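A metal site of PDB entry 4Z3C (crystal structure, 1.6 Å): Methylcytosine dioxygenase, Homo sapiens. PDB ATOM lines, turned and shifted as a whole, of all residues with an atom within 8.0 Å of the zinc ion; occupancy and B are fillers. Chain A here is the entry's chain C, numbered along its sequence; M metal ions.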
ATOM      1  N   ARG A  19      -1.783  26.692 -29.025  1.00  0.00           N
ATOM      2  CA  ARG A  19      -2.308  25.339 -28.981  1.00  0.00           C
ATOM      3  C   ARG A  19      -3.855  25.391 -28.946  1.00  0.00           C
ATOM      4  O   ARG A  19      -4.433  26.252 -28.316  1.00  0.00           O
ATOM      5  CB  ARG A  19      -1.712  24.591 -27.769  1.00  0.00           C
ATOM      6  CG  ARG A  19      -1.787  23.104 -27.921  1.00  0.00           C
ATOM      7  CD  ARG A  19      -1.366  22.359 -26.662  1.00  0.00           C
ATOM      8  NE  ARG A  19       0.083  22.349 -26.476  1.00  0.00           N
ATOM      9  CZ  ARG A  19       0.797  21.232 -26.313  1.00  0.00           C
ATOM     10  NH1 ARG A  19       2.114  21.303 -26.157  1.00  0.00           N
ATOM     11  NH2 ARG A  19       0.190  20.047 -26.297  1.00  0.00           N
ATOM     12  N   GLU A  21      -5.750  22.208 -28.535  1.00  0.00           N
ATOM     13  CA  GLU A  21      -6.280  21.075 -27.802  1.00  0.00           C
ATOM     14  C   GLU A  21      -5.795  21.041 -26.363  1.00  0.00           C
ATOM     15  O   GLU A  21      -4.640  21.238 -26.120  1.00  0.00           O
ATOM     16  CB  GLU A  21      -5.870  19.756 -28.511  1.00  0.00           C
ATOM     17  CG  GLU A  21      -6.392  19.622 -29.938  1.00  0.00           C
ATOM     18  N   ASN A  22      -6.695  20.685 -25.444  1.00  0.00           N
ATOM     19  CA  ASN A  22      -6.330  20.294 -24.064  1.00  0.00           C
ATOM     20  C   ASN A  22      -5.637  18.965 -24.061  1.00  0.00           C
ATOM     21  O   ASN A  22      -6.072  18.041 -24.779  1.00  0.00           O
ATOM     22  CB  ASN A  22      -7.537  20.174 -23.195  1.00  0.00           C
ATOM     23  CG  ASN A  22      -8.205  21.475 -22.947  1.00  0.00           C
ATOM     24  OD1 ASN A  22      -7.561  22.505 -22.882  1.00  0.00           O
ATOM     25  ND2 ASN A  22      -9.558  21.453 -22.883  1.00  0.00           N
ATOM     26  N   CYS A  23      -4.572  18.813 -23.250  1.00  0.00           N
ATOM     27  CA  CYS A  23      -3.773  17.565 -23.258  1.00  0.00           C
ATOM     28  C   CYS A  23      -4.525  16.288 -22.741  1.00  0.00           C
ATOM     29  O   CYS A  23      -4.275  15.149 -23.183  1.00  0.00           O
ATOM     30  CB  CYS A  23      -2.414  17.722 -22.493  1.00  0.00           C
ATOM     31  SG  CYS A  23      -2.404  17.673 -20.721  1.00  0.00           S
ATOM     32  N   GLY A  24      -5.418  16.515 -21.783  1.00  0.00           N
ATOM     33  CA  GLY A  24      -6.165  15.435 -21.135  1.00  0.00           C
ATOM     34  C   GLY A  24      -5.544  14.788 -19.919  1.00  0.00           C
ATOM     35  O   GLY A  24      -6.232  13.989 -19.274  1.00  0.00           O
ATOM     36  N   ALA A  25      -4.273  15.074 -19.647  1.00  0.00           N
ATOM     37  CA  ALA A  25      -3.445  14.314 -18.641  1.00  0.00           C
ATOM     38  C   ALA A  25      -2.860  15.086 -17.471  1.00  0.00           C
ATOM     39  O   ALA A  25      -2.395  14.487 -16.486  1.00  0.00           O
ATOM     40  CB  ALA A  25      -2.304  13.606 -19.349  1.00  0.00           C
ATOM     41  N   CYS A  26      -2.816  16.432 -17.587  1.00  0.00           N
ATOM     42  CA  CYS A  26      -2.287  17.302 -16.489  1.00  0.00           C
ATOM     43  C   CYS A  26      -3.308  17.474 -15.431  1.00  0.00           C
ATOM     44  O   CYS A  26      -4.478  17.075 -15.609  1.00  0.00           O
ATOM     45  CB  CYS A  26      -1.804  18.679 -17.030  1.00  0.00           C
ATOM     46  SG  CYS A  26      -3.128  19.663 -17.729  1.00  0.00           S
ATOM     47  N   THR A  27      -2.894  18.060 -14.304  1.00  0.00           N
ATOM     48  CA  THR A  27      -3.800  18.406 -13.210  1.00  0.00           C
ATOM     49  C   THR A  27      -4.988  19.197 -13.637  1.00  0.00           C
ATOM     50  O   THR A  27      -6.041  18.966 -13.151  1.00  0.00           O
ATOM     51  CB  THR A  27      -3.091  19.262 -12.114  1.00  0.00           C
ATOM     52  OG1 THR A  27      -2.204  20.218 -12.725  1.00  0.00           O
ATOM     53  CG2 THR A  27      -2.311  18.437 -11.291  1.00  0.00           C
ATOM     54  N   SER A  28      -4.804  20.175 -14.564  1.00  0.00           N
ATOM     55  CA  SER A  28      -5.887  20.952 -15.005  1.00  0.00           C
ATOM     56  C   SER A  28      -6.916  20.128 -15.708  1.00  0.00           C
ATOM     57  O   SER A  28      -8.056  20.219 -15.435  1.00  0.00           O
ATOM     58  CB  SER A  28      -5.392  21.987 -15.962  1.00  0.00           C
ATOM     59  OG  SER A  28      -4.481  22.798 -15.280  1.00  0.00           O
ATOM     60  N   CYS A  29      -6.435  19.307 -16.642  1.00  0.00           N
ATOM     61  CA  CYS A  29      -7.278  18.569 -17.530  1.00  0.00           C
ATOM     62  C   CYS A  29      -7.950  17.447 -16.781  1.00  0.00           C
ATOM     63  O   CYS A  29      -9.065  17.100 -17.093  1.00  0.00           O
ATOM     64  CB  CYS A  29      -6.513  18.010 -18.713  1.00  0.00           C
ATOM     65  SG  CYS A  29      -6.085  19.245 -19.937  1.00  0.00           S
ATOM     66  N   THR A  30      -7.288  16.863 -15.787  1.00  0.00           N
ATOM     67  CA  THR A  30      -7.939  15.744 -15.050  1.00  0.00           C
ATOM     68  C   THR A  30      -8.683  16.165 -13.816  1.00  0.00           C
ATOM     69  O   THR A  30      -9.570  15.500 -13.387  1.00  0.00           O
ATOM     70  CB  THR A  30      -6.911  14.668 -14.634  1.00  0.00           C
ATOM     71  OG1 THR A  30      -5.860  15.269 -13.885  1.00  0.00           O
ATOM     72  CG2 THR A  30      -6.324  14.048 -15.823  1.00  0.00           C
ATOM     73  N   GLN A  36      -8.422  25.458 -13.791  1.00  0.00           N
ATOM     74  CA  GLN A  36      -7.299  25.969 -14.584  1.00  0.00           C
ATOM     75  C   GLN A  36      -7.281  25.531 -16.046  1.00  0.00           C
ATOM     76  O   GLN A  36      -7.828  24.492 -16.420  1.00  0.00           O
ATOM     77  CB  GLN A  36      -5.969  25.585 -13.914  1.00  0.00           C
ATOM     78  CG  GLN A  36      -5.753  26.064 -12.477  1.00  0.00           C
ATOM     79  CD  GLN A  36      -5.805  27.614 -12.256  1.00  0.00           C
ATOM     80  OE1 GLN A  36      -5.176  28.400 -12.959  1.00  0.00           O
ATOM     81  NE2 GLN A  36      -6.544  28.027 -11.228  1.00  0.00           N
ATOM     82  N   ILE A  37      -6.606  26.321 -16.872  1.00  0.00           N
ATOM     83  CA  ILE A  37      -6.358  25.942 -18.206  1.00  0.00           C
ATOM     84  C   ILE A  37      -5.371  24.804 -18.257  1.00  0.00           C
ATOM     85  O   ILE A  37      -4.523  24.703 -17.368  1.00  0.00           O
ATOM     86  CB  ILE A  37      -5.822  27.161 -19.017  1.00  0.00           C
ATOM     87  CG1 ILE A  37      -5.942  26.910 -20.513  1.00  0.00           C
ATOM     88  CG2 ILE A  37      -4.408  27.567 -18.608  1.00  0.00           C
ATOM     89  CD1 ILE A  37      -5.500  28.074 -21.365  1.00  0.00           C
ATOM     90  N   CYS A  38      -5.506  23.931 -19.260  1.00  0.00           N
ATOM     91  CA  CYS A  38      -4.457  22.914 -19.539  1.00  0.00           C
ATOM     92  C   CYS A  38      -3.040  23.467 -19.345  1.00  0.00           C
ATOM     93  O   CYS A  38      -2.689  24.528 -19.831  1.00  0.00           O
ATOM     94  CB  CYS A  38      -4.584  22.415 -20.986  1.00  0.00           C
ATOM     95  SG  CYS A  38      -3.295  21.197 -21.385  1.00  0.00           S
ATOM     96  N   LYS A  39      -2.181  22.786 -18.598  1.00  0.00           N
ATOM     97  CA  LYS A  39      -0.817  23.250 -18.292  1.00  0.00           C
ATOM     98  C   LYS A  39       0.018  23.560 -19.549  1.00  0.00           C
ATOM     99  O   LYS A  39       0.823  24.528 -19.567  1.00  0.00           O
ATOM    100  CB  LYS A  39      -0.095  22.207 -17.377  1.00  0.00           C
ATOM    101  CG  LYS A  39      -0.692  22.189 -15.974  1.00  0.00           C
ATOM    102  CD  LYS A  39       0.228  21.458 -14.994  1.00  0.00           C
ATOM    103  N   LEU A  40      -0.270  22.853 -20.637  1.00  0.00           N
ATOM    104  CA  LEU A  40       0.483  23.034 -21.887  1.00  0.00           C
ATOM    105  C   LEU A  40      -0.031  24.241 -22.690  1.00  0.00           C
ATOM    106  O   LEU A  40       0.610  24.660 -23.650  1.00  0.00           O
ATOM    107  CB  LEU A  40       0.435  21.762 -22.736  1.00  0.00           C
ATOM    108  CG  LEU A  40       1.095  20.573 -22.044  1.00  0.00           C
ATOM    109  CD1 LEU A  40       1.072  19.363 -22.963  1.00  0.00           C
ATOM    110  CD2 LEU A  40       2.513  20.959 -21.625  1.00  0.00           C
ATOM    111  N   ARG A  41      -1.161  24.776 -22.261  1.00  0.00           N
ATOM    112  CA  ARG A  41      -1.842  25.891 -22.926  1.00  0.00           C
ATOM    113  C   ARG A  41      -1.714  27.206 -22.140  1.00  0.00           C
ATOM    114  O   ARG A  41      -1.945  28.261 -22.691  1.00  0.00           O
ATOM    115  CB  ARG A  41      -3.284  25.573 -23.124  1.00  0.00           C
ATOM    116  CG  ARG A  41      -3.529  24.380 -23.980  1.00  0.00           C
ATOM    117  CD  ARG A  41      -4.979  24.195 -24.195  1.00  0.00           C
ATOM    118  NE  ARG A  41      -5.490  25.127 -25.181  1.00  0.00           N
ATOM    119  CZ  ARG A  41      -6.732  25.135 -25.643  1.00  0.00           C
ATOM    120  NH1 ARG A  41      -7.065  26.025 -26.574  1.00  0.00           N
ATOM    121  NH2 ARG A  41      -7.654  24.244 -25.229  1.00  0.00           N
HETATM  122 ZN    ZN M   1      -3.660  19.423 -19.997  1.00  0.00          ZN
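SG of Cys 23 is bound to the zinc ion (2.3 Å).
SG of Cys 38 binds the zinc ion.
SG of Cys 26 is bound to the zinc ion (2.3 Å).
The zinc ion is bound by the side-chain sulfur (SG) of Cys 29, at 2.4 Å.
The side-chain hydroxyl of Thr 30 lies within hydrogen-bond range of the backbone carbonyl oxygen of Cys 26, 2.9 Å away.
The side-chain sulfur (SG) of Cys 29 sits close to the backbone NH (N) of Gly 24, 3.4 Å away.
The backbone NH (N) of Ser 28 lies close to the side-chain sulfur (SG) of Cys 26 (3.6 Å).
SG of Cys 38 lies close to N of Leu 40, at 3.5 Å.
SG of Cys 23 sits close to N of Ala 25 (3.4 Å).
The backbone NH (N) of Lys 39 lies close to the side-chain sulfur (SG) of Cys 26, 3.4 Å away.
Merely in contact with the zinc ion: Gly 24 (3.8 Å) and Lys 39 (3.9 Å).
The nearest printed residue that does not touch the zinc ion is Ala 25 (4.4 Å).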
